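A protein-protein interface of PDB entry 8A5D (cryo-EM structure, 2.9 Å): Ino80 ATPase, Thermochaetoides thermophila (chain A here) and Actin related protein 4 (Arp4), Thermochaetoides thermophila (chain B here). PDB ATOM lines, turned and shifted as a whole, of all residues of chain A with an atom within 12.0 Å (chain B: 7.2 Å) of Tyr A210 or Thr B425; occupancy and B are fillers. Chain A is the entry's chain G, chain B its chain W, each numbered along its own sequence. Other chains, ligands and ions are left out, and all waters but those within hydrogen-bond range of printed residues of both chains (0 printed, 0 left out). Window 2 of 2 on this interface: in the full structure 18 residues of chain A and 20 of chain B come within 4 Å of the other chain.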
ATOM      1  N   LYS A 201      21.356 -35.738 -29.711  1.00  0.00           N
ATOM      2  CA  LYS A 201      20.022 -35.294 -29.230  1.00  0.00           C
ATOM      3  C   LYS A 201      20.188 -34.008 -28.423  1.00  0.00           C
ATOM      4  O   LYS A 201      19.417 -33.039 -28.670  1.00  0.00           O
ATOM      5  CB  LYS A 201      19.314 -36.369 -28.406  1.00  0.00           C
ATOM      6  CG  LYS A 201      18.628 -37.423 -29.259  1.00  0.00           C
ATOM      7  CD  LYS A 201      17.915 -38.508 -28.460  1.00  0.00           C
ATOM      8  CE  LYS A 201      17.113 -39.468 -29.321  1.00  0.00           C
ATOM      9  NZ  LYS A 201      16.515 -40.568 -28.528  1.00  0.00           N
ATOM     10  N   VAL A 202      21.139 -33.977 -27.497  1.00  0.00           N
ATOM     11  CA  VAL A 202      21.213 -32.852 -26.531  1.00  0.00           C
ATOM     12  C   VAL A 202      21.740 -31.586 -27.194  1.00  0.00           C
ATOM     13  O   VAL A 202      21.229 -30.501 -26.869  1.00  0.00           O
ATOM     14  CB  VAL A 202      21.949 -33.238 -25.257  1.00  0.00           C
ATOM     15  CG1 VAL A 202      22.014 -32.062 -24.305  1.00  0.00           C
ATOM     16  CG2 VAL A 202      21.180 -34.381 -24.583  1.00  0.00           C
ATOM     17  N   PHE A 203      22.582 -31.697 -28.190  1.00  0.00           N
ATOM     18  CA  PHE A 203      22.933 -30.540 -29.041  1.00  0.00           C
ATOM     19  C   PHE A 203      21.734 -29.949 -29.786  1.00  0.00           C
ATOM     20  O   PHE A 203      21.605 -28.720 -29.785  1.00  0.00           O
ATOM     21  CB  PHE A 203      24.008 -30.953 -29.997  1.00  0.00           C
ATOM     22  CG  PHE A 203      24.461 -29.865 -30.884  1.00  0.00           C
ATOM     23  CD1 PHE A 203      25.446 -28.992 -30.446  1.00  0.00           C
ATOM     24  CD2 PHE A 203      23.962 -29.770 -32.162  1.00  0.00           C
ATOM     25  CE1 PHE A 203      25.917 -28.004 -31.293  1.00  0.00           C
ATOM     26  CE2 PHE A 203      24.447 -28.796 -33.009  1.00  0.00           C
ATOM     27  CZ  PHE A 203      25.419 -27.919 -32.570  1.00  0.00           C
ATOM     28  N   ARG A 204      20.827 -30.749 -30.323  1.00  0.00           N
ATOM     29  CA  ARG A 204      19.629 -30.206 -31.036  1.00  0.00           C
ATOM     30  C   ARG A 204      18.707 -29.530 -30.014  1.00  0.00           C
ATOM     31  O   ARG A 204      18.241 -28.417 -30.263  1.00  0.00           O
ATOM     32  CB  ARG A 204      18.879 -31.300 -31.788  1.00  0.00           C
ATOM     33  CG  ARG A 204      17.780 -30.757 -32.686  1.00  0.00           C
ATOM     34  CD  ARG A 204      16.995 -31.858 -33.365  1.00  0.00           C
ATOM     35  NE  ARG A 204      16.342 -31.408 -34.593  1.00  0.00           N
ATOM     36  CZ  ARG A 204      15.907 -32.200 -35.576  1.00  0.00           C
ATOM     37  NH1 ARG A 204      16.040 -33.517 -35.510  1.00  0.00           N
ATOM     38  NH2 ARG A 204      15.332 -31.661 -36.640  1.00  0.00           N
ATOM     39  N   LEU A 205      18.476 -30.165 -28.873  1.00  0.00           N
ATOM     40  CA  LEU A 205      17.625 -29.609 -27.796  1.00  0.00           C
ATOM     41  C   LEU A 205      18.236 -28.287 -27.316  1.00  0.00           C
ATOM     42  O   LEU A 205      17.480 -27.316 -27.179  1.00  0.00           O
ATOM     43  CB  LEU A 205      17.534 -30.666 -26.701  1.00  0.00           C
ATOM     44  CG  LEU A 205      16.705 -30.316 -25.472  1.00  0.00           C
ATOM     45  CD1 LEU A 205      16.047 -31.579 -24.930  1.00  0.00           C
ATOM     46  CD2 LEU A 205      17.556 -29.650 -24.394  1.00  0.00           C
ATOM     47  N   ALA A 206      19.536 -28.236 -27.061  1.00  0.00           N
ATOM     48  CA  ALA A 206      20.221 -27.024 -26.570  1.00  0.00           C
ATOM     49  C   ALA A 206      20.146 -25.893 -27.628  1.00  0.00           C
ATOM     50  O   ALA A 206      19.891 -24.767 -27.249  1.00  0.00           O
ATOM     51  CB  ALA A 206      21.641 -27.349 -26.157  1.00  0.00           C
ATOM     52  N   THR A 207      20.358 -26.150 -28.898  1.00  0.00           N
ATOM     53  CA  THR A 207      20.390 -25.097 -29.924  1.00  0.00           C
ATOM     54  C   THR A 207      18.975 -24.545 -30.081  1.00  0.00           C
ATOM     55  O   THR A 207      18.824 -23.294 -30.237  1.00  0.00           O
ATOM     56  CB  THR A 207      20.995 -25.563 -31.259  1.00  0.00           C
ATOM     57  OG1 THR A 207      20.336 -26.754 -31.671  1.00  0.00           O
ATOM     58  CG2 THR A 207      22.491 -25.834 -31.189  1.00  0.00           C
ATOM     59  N   ASP A 208      17.959 -25.399 -30.064  1.00  0.00           N
ATOM     60  CA  ASP A 208      16.547 -24.930 -30.142  1.00  0.00           C
ATOM     61  C   ASP A 208      16.224 -24.151 -28.866  1.00  0.00           C
ATOM     62  O   ASP A 208      15.583 -23.112 -28.971  1.00  0.00           O
ATOM     63  CB  ASP A 208      15.567 -26.085 -30.344  1.00  0.00           C
ATOM     64  CG  ASP A 208      15.639 -26.737 -31.718  1.00  0.00           C
ATOM     65  OD1 ASP A 208      16.298 -26.165 -32.620  1.00  0.00           O
ATOM     66  OD2 ASP A 208      15.005 -27.805 -31.885  1.00  0.00           O
ATOM     67  N   SER A 209      16.609 -24.659 -27.702  1.00  0.00           N
ATOM     68  CA  SER A 209      16.327 -24.019 -26.398  1.00  0.00           C
ATOM     69  C   SER A 209      16.916 -22.612 -26.399  1.00  0.00           C
ATOM     70  O   SER A 209      16.180 -21.677 -26.055  1.00  0.00           O
ATOM     71  CB  SER A 209      16.805 -24.851 -25.233  1.00  0.00           C
ATOM     72  OG  SER A 209      16.552 -24.219 -23.975  1.00  0.00           O
ATOM     73  N   TYR A 210      18.183 -22.452 -26.734  1.00  0.00           N
ATOM     74  CA  TYR A 210      18.831 -21.120 -26.843  1.00  0.00           C
ATOM     75  C   TYR A 210      18.034 -20.178 -27.780  1.00  0.00           C
ATOM     76  O   TYR A 210      17.793 -19.047 -27.375  1.00  0.00           O
ATOM     77  CB  TYR A 210      20.289 -21.232 -27.300  1.00  0.00           C
ATOM     78  CG  TYR A 210      20.908 -19.882 -27.456  1.00  0.00           C
ATOM     79  CD1 TYR A 210      21.316 -19.207 -26.324  1.00  0.00           C
ATOM     80  CD2 TYR A 210      20.953 -19.220 -28.683  1.00  0.00           C
ATOM     81  CE1 TYR A 210      21.843 -17.924 -26.406  1.00  0.00           C
ATOM     82  CE2 TYR A 210      21.451 -17.926 -28.780  1.00  0.00           C
ATOM     83  CZ  TYR A 210      21.896 -17.273 -27.635  1.00  0.00           C
ATOM     84  OH  TYR A 210      22.405 -16.003 -27.713  1.00  0.00           O
ATOM     85  N   ALA A 211      17.620 -20.609 -28.955  1.00  0.00           N
ATOM     86  CA  ALA A 211      16.803 -19.802 -29.887  1.00  0.00           C
ATOM     87  C   ALA A 211      15.473 -19.369 -29.244  1.00  0.00           C
ATOM     88  O   ALA A 211      15.085 -18.216 -29.432  1.00  0.00           O
ATOM     89  CB  ALA A 211      16.556 -20.564 -31.169  1.00  0.00           C
ATOM     90  N   THR A 212      14.828 -20.219 -28.454  1.00  0.00           N
ATOM     91  CA  THR A 212      13.580 -19.888 -27.724  1.00  0.00           C
ATOM     92  C   THR A 212      13.906 -18.859 -26.639  1.00  0.00           C
ATOM     93  O   THR A 212      13.159 -17.874 -26.534  1.00  0.00           O
ATOM     94  CB  THR A 212      12.922 -21.130 -27.115  1.00  0.00           C
ATOM     95  OG1 THR A 212      12.597 -21.969 -28.224  1.00  0.00           O
ATOM     96  CG2 THR A 212      11.680 -20.826 -26.313  1.00  0.00           C
ATOM     97  N   LYS A 213      14.972 -19.063 -25.871  1.00  0.00           N
ATOM     98  CA  LYS A 213      15.340 -18.157 -24.756  1.00  0.00           C
ATOM     99  C   LYS A 213      15.627 -16.776 -25.344  1.00  0.00           C
ATOM    100  O   LYS A 213      15.034 -15.802 -24.899  1.00  0.00           O
ATOM    101  CB  LYS A 213      16.495 -18.764 -23.991  1.00  0.00           C
ATOM    102  CG  LYS A 213      17.177 -17.905 -22.954  1.00  0.00           C
ATOM    103  CD  LYS A 213      18.454 -18.541 -22.408  1.00  0.00           C
ATOM    104  CE  LYS A 213      19.150 -17.627 -21.426  1.00  0.00           C
ATOM    105  NZ  LYS A 213      20.170 -18.300 -20.582  1.00  0.00           N
ATOM    106  N   ALA A 214      16.485 -16.685 -26.333  1.00  0.00           N
ATOM    107  CA  ALA A 214      16.820 -15.410 -26.992  1.00  0.00           C
ATOM    108  C   ALA A 214      15.571 -14.747 -27.579  1.00  0.00           C
ATOM    109  O   ALA A 214      15.451 -13.512 -27.426  1.00  0.00           O
ATOM    110  CB  ALA A 214      17.851 -15.667 -28.045  1.00  0.00           C
ATOM    111  N   SER A 215      14.665 -15.487 -28.218  1.00  0.00           N
ATOM    112  CA  SER A 215      13.404 -14.937 -28.808  1.00  0.00           C
ATOM    113  C   SER A 215      12.485 -14.388 -27.719  1.00  0.00           C
ATOM    114  O   SER A 215      12.076 -13.237 -27.851  1.00  0.00           O
ATOM    115  CB  SER A 215      12.695 -15.962 -29.633  1.00  0.00           C
ATOM    116  OG  SER A 215      11.363 -15.567 -29.965  1.00  0.00           O
ATOM    117  N   ASN A 216      12.261 -15.152 -26.640  1.00  0.00           N
ATOM    118  CA  ASN A 216      11.443 -14.759 -25.468  1.00  0.00           C
ATOM    119  C   ASN A 216      11.921 -13.402 -24.926  1.00  0.00           C
ATOM    120  O   ASN A 216      11.091 -12.490 -24.693  1.00  0.00           O
ATOM    121  CB  ASN A 216      11.565 -15.804 -24.362  1.00  0.00           C
ATOM    122  CG  ASN A 216      10.688 -17.023 -24.509  1.00  0.00           C
ATOM    123  OD1 ASN A 216       9.884 -17.141 -25.433  1.00  0.00           O
ATOM    124  ND2 ASN A 216      10.773 -17.906 -23.525  1.00  0.00           N
ATOM    125  N   LEU A 217      13.219 -13.302 -24.713  1.00  0.00           N
ATOM    126  CA  LEU A 217      13.851 -12.138 -24.059  1.00  0.00           C
ATOM    127  C   LEU A 217      13.750 -10.947 -25.012  1.00  0.00           C
ATOM    128  O   LEU A 217      13.458  -9.841 -24.520  1.00  0.00           O
ATOM    129  CB  LEU A 217      15.334 -12.390 -23.750  1.00  0.00           C
ATOM    130  CG  LEU A 217      15.587 -13.480 -22.732  1.00  0.00           C
ATOM    131  CD1 LEU A 217      17.064 -13.550 -22.389  1.00  0.00           C
ATOM    132  CD2 LEU A 217      14.716 -13.307 -21.508  1.00  0.00           C
ATOM    133  N   LYS A 218      13.999 -11.127 -26.304  1.00  0.00           N
ATOM    134  CA  LYS A 218      14.072  -9.988 -27.226  1.00  0.00           C
ATOM    135  C   LYS A 218      12.672  -9.371 -27.228  1.00  0.00           C
ATOM    136  O   LYS A 218      12.578  -8.156 -27.111  1.00  0.00           O
ATOM    137  CB  LYS A 218      14.519 -10.431 -28.623  1.00  0.00           C
ATOM    138  CG  LYS A 218      14.571  -9.329 -29.662  1.00  0.00           C
ATOM    139  CD  LYS A 218      14.586  -9.835 -31.065  1.00  0.00           C
ATOM    140  CE  LYS A 218      14.923  -8.736 -32.063  1.00  0.00           C
ATOM    141  NZ  LYS A 218      15.156  -9.264 -33.437  1.00  0.00           N
ATOM    142  N   LYS A 219      11.626 -10.152 -27.463  1.00  0.00           N
ATOM    143  CA  LYS A 219      10.266  -9.603 -27.628  1.00  0.00           C
ATOM    144  C   LYS A 219       9.842  -8.955 -26.298  1.00  0.00           C
ATOM    145  O   LYS A 219       9.208  -7.906 -26.324  1.00  0.00           O
ATOM    146  CB  LYS A 219       9.326 -10.686 -28.176  1.00  0.00           C
ATOM    147  CG  LYS A 219       7.905 -10.243 -28.518  1.00  0.00           C
ATOM    148  CD  LYS A 219       7.815  -9.280 -29.702  1.00  0.00           C
ATOM    149  CE  LYS A 219       6.492  -9.287 -30.458  1.00  0.00           C
ATOM    150  NZ  LYS A 219       6.428  -8.215 -31.485  1.00  0.00           N
ATOM    151  N   GLU B  41      24.985 -22.135 -21.707  1.00  0.00           N
ATOM    152  CA  GLU B  41      25.402 -21.960 -23.106  1.00  0.00           C
ATOM    153  C   GLU B  41      26.759 -21.288 -23.180  1.00  0.00           C
ATOM    154  O   GLU B  41      27.307 -21.395 -24.304  1.00  0.00           O
ATOM    155  CB  GLU B  41      24.421 -21.098 -23.900  1.00  0.00           C
ATOM    156  CG  GLU B  41      22.989 -21.612 -23.874  1.00  0.00           C
ATOM    157  CD  GLU B  41      22.069 -21.051 -22.790  1.00  0.00           C
ATOM    158  OE1 GLU B  41      22.574 -20.344 -21.877  1.00  0.00           O
ATOM    159  OE2 GLU B  41      20.829 -21.319 -22.863  1.00  0.00           O
ATOM    160  N   MET B  42      27.213 -20.563 -22.137  1.00  0.00           N
ATOM    161  CA  MET B  42      28.544 -19.900 -22.134  1.00  0.00           C
ATOM    162  C   MET B  42      29.130 -19.832 -20.748  1.00  0.00           C
ATOM    163  O   MET B  42      28.397 -19.919 -19.766  1.00  0.00           O
ATOM    164  CB  MET B  42      28.385 -18.498 -22.684  1.00  0.00           C
ATOM    165  CG  MET B  42      28.232 -18.474 -24.215  1.00  0.00           C
ATOM    166  SD  MET B  42      28.350 -16.808 -24.872  1.00  0.00           S
ATOM    167  CE  MET B  42      26.929 -16.034 -24.083  1.00  0.00           C
ATOM    168  N   ALA B 187      30.700 -30.027 -28.908  1.00  0.00           N
ATOM    169  CA  ALA B 187      30.240 -28.634 -29.089  1.00  0.00           C
ATOM    170  C   ALA B 187      29.697 -28.390 -30.496  1.00  0.00           C
ATOM    171  O   ALA B 187      28.915 -27.446 -30.640  1.00  0.00           O
ATOM    172  CB  ALA B 187      31.338 -27.669 -28.739  1.00  0.00           C
ATOM    173  N   ALA B 421      31.014 -24.970 -37.098  1.00  0.00           N
ATOM    174  CA  ALA B 421      31.496 -24.191 -35.942  1.00  0.00           C
ATOM    175  C   ALA B 421      31.256 -25.017 -34.679  1.00  0.00           C
ATOM    176  O   ALA B 421      30.173 -25.593 -34.532  1.00  0.00           O
ATOM    177  CB  ALA B 421      30.750 -22.887 -35.923  1.00  0.00           C
ATOM    178  N   ALA B 422      32.191 -25.022 -33.745  1.00  0.00           N
ATOM    179  CA  ALA B 422      31.897 -25.431 -32.350  1.00  0.00           C
ATOM    180  C   ALA B 422      31.024 -24.342 -31.710  1.00  0.00           C
ATOM    181  O   ALA B 422      31.363 -23.143 -31.824  1.00  0.00           O
ATOM    182  CB  ALA B 422      33.191 -25.613 -31.607  1.00  0.00           C
ATOM    183  N   GLY B 423      29.940 -24.709 -31.050  1.00  0.00           N
ATOM    184  CA  GLY B 423      29.115 -23.709 -30.356  1.00  0.00           C
ATOM    185  C   GLY B 423      27.646 -23.738 -30.773  1.00  0.00           C
ATOM    186  O   GLY B 423      27.302 -24.114 -31.929  1.00  0.00           O
ATOM    187  N   LEU B 424      26.804 -23.299 -29.846  1.00  0.00           N
ATOM    188  CA  LEU B 424      25.335 -23.277 -29.964  1.00  0.00           C
ATOM    189  C   LEU B 424      24.899 -22.025 -30.726  1.00  0.00           C
ATOM    190  O   LEU B 424      23.751 -22.000 -31.195  1.00  0.00           O
ATOM    191  CB  LEU B 424      24.759 -23.323 -28.541  1.00  0.00           C
ATOM    192  CG  LEU B 424      25.121 -24.601 -27.775  1.00  0.00           C
ATOM    193  CD1 LEU B 424      24.725 -24.520 -26.313  1.00  0.00           C
ATOM    194  CD2 LEU B 424      24.441 -25.800 -28.427  1.00  0.00           C
ATOM    195  N   THR B 425      25.781 -21.031 -30.852  1.00  0.00           N
ATOM    196  CA  THR B 425      25.448 -19.604 -31.126  1.00  0.00           C
ATOM    197  C   THR B 425      26.460 -19.040 -32.137  1.00  0.00           C
ATOM    198  O   THR B 425      27.486 -19.712 -32.407  1.00  0.00           O
ATOM    199  CB  THR B 425      25.455 -18.818 -29.799  1.00  0.00           C
ATOM    200  OG1 THR B 425      24.624 -19.452 -28.825  1.00  0.00           O
ATOM    201  CG2 THR B 425      24.966 -17.389 -29.920  1.00  0.00           C
ATOM    202  N   SER B 426      26.227 -17.830 -32.644  1.00  0.00           N
ATOM    203  CA  SER B 426      27.211 -17.060 -33.447  1.00  0.00           C
ATOM    204  C   SER B 426      28.484 -16.760 -32.622  1.00  0.00           C
ATOM    205  O   SER B 426      29.553 -16.527 -33.234  1.00  0.00           O
ATOM    206  CB  SER B 426      26.577 -15.811 -33.989  1.00  0.00           C
ATOM    207  OG  SER B 426      27.432 -15.190 -34.936  1.00  0.00           O
ATOM    208  N   GLU B 427      28.416 -16.787 -31.288  1.00  0.00           N
ATOM    209  CA  GLU B 427      29.609 -16.718 -30.400  1.00  0.00           C
ATOM    210  C   GLU B 427      30.422 -18.010 -30.512  1.00  0.00           C
ATOM    211  O   GLU B 427      29.913 -19.061 -30.069  1.00  0.00           O
ATOM    212  CB  GLU B 427      29.222 -16.500 -28.936  1.00  0.00           C
ATOM    213  CG  GLU B 427      30.416 -16.415 -27.994  1.00  0.00           C
ATOM    214  CD  GLU B 427      31.444 -15.363 -28.372  1.00  0.00           C
ATOM    215  OE1 GLU B 427      31.245 -14.176 -28.026  1.00  0.00           O
ATOM    216  OE2 GLU B 427      32.442 -15.729 -29.038  1.00  0.00           O
ATOM    217  N   ARG B 428      31.648 -17.922 -31.043  1.00  0.00           N
ATOM    218  CA  ARG B 428      32.548 -19.075 -31.281  1.00  0.00           C
ATOM    219  C   ARG B 428      33.897 -18.970 -30.523  1.00  0.00           C
ATOM    220  O   ARG B 428      34.791 -19.743 -30.813  1.00  0.00           O
ATOM    221  CB  ARG B 428      32.733 -19.130 -32.798  1.00  0.00           C
ATOM    222  CG  ARG B 428      31.475 -19.490 -33.566  1.00  0.00           C
ATOM    223  CD  ARG B 428      31.711 -19.506 -35.058  1.00  0.00           C
ATOM    224  NE  ARG B 428      31.942 -18.177 -35.605  1.00  0.00           N
ATOM    225  CZ  ARG B 428      32.828 -17.865 -36.560  1.00  0.00           C
ATOM    226  NH1 ARG B 428      33.614 -18.783 -37.111  1.00  0.00           N
ATOM    227  NH2 ARG B 428      32.929 -16.606 -36.961  1.00  0.00           N
ATOM    228  N   ILE B 434      32.048 -25.278 -24.113  1.00  0.00           N
ATOM    229  CA  ILE B 434      30.590 -25.640 -24.333  1.00  0.00           C
ATOM    230  C   ILE B 434      30.444 -27.152 -24.448  1.00  0.00           C
ATOM    231  O   ILE B 434      29.421 -27.678 -24.013  1.00  0.00           O
ATOM    232  CB  ILE B 434      30.039 -24.937 -25.589  1.00  0.00           C
ATOM    233  CG1 ILE B 434      29.974 -23.422 -25.375  1.00  0.00           C
ATOM    234  CG2 ILE B 434      28.699 -25.512 -26.014  1.00  0.00           C
ATOM    235  CD1 ILE B 434      29.672 -22.638 -26.626  1.00  0.00           C
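The side-chain carboxylate (OE1) of Glu B41 lies within salt-bridge range of the side-chain amino group (NZ) of Lys A213 (3.4 Å).
The side-chain hydroxyl (OG1) of Thr A207 sits at hydrogen-bond distance from the backbone carbonyl oxygen (O) of Phe A203, at 3.0 Å. The side-chain hydroxyl (OG1) of Thr A207 is in hydrogen-bond range of the backbone carbonyl oxygen (O) of Arg A204 (3.0 Å). N of Gly B423 is in hydrogen-bond range of O of Ala B187.
Among the printed residues, pairs that only touch across the chains: Phe A203 with Ala B187 (3.1 Å), Thr A207 with Leu B424 (3.4 Å), Tyr A210 with Thr B425 (3.5 Å), Tyr A210 with Glu B41 (3.8 Å), Phe A203 with Leu B424 (3.9 Å) and Ala A206 with Leu B424 (3.9 Å).
Val A202 touches none of the printed residues of chain B. Leu A205 touches none of the printed residues of chain B. Printed residues of chain B within 4 Å of Thr A207: Leu B424 (3.4 Å). Tyr A210 touches just these residues of chain B: Glu B41 (3.8 Å) and Thr B425 (3.5 Å). Of the printed residues of chain B, Lys A213 touches Glu B41 (3.4 Å). Glu B41 touches just these residues of chain A: Tyr A210 (3.8 Å) and Lys A213 (3.4 Å). Of the printed residues of chain A, Ala B187 touches Phe A203. No residue of chain A comes within 4 Å of Ala B421. No residue of chain A comes within 4 Å of Gly B423. Thr B425 touches one residue of chain A. No residue of chain A comes within 4 Å of Arg B428.
Hydrophobic or aromatic side chains of chain B within 4 Å of the printed part of chain A: Leu B424. Hydrophobic or aromatic side chains of chain A that line the printed part of chain B: Phe A203, Ala A206 and Tyr A210. Along chain A the printed residues that touch a printed residue of chain B span positions 203 to 213. Among the printed residues, 7 pairs touch across the chains.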
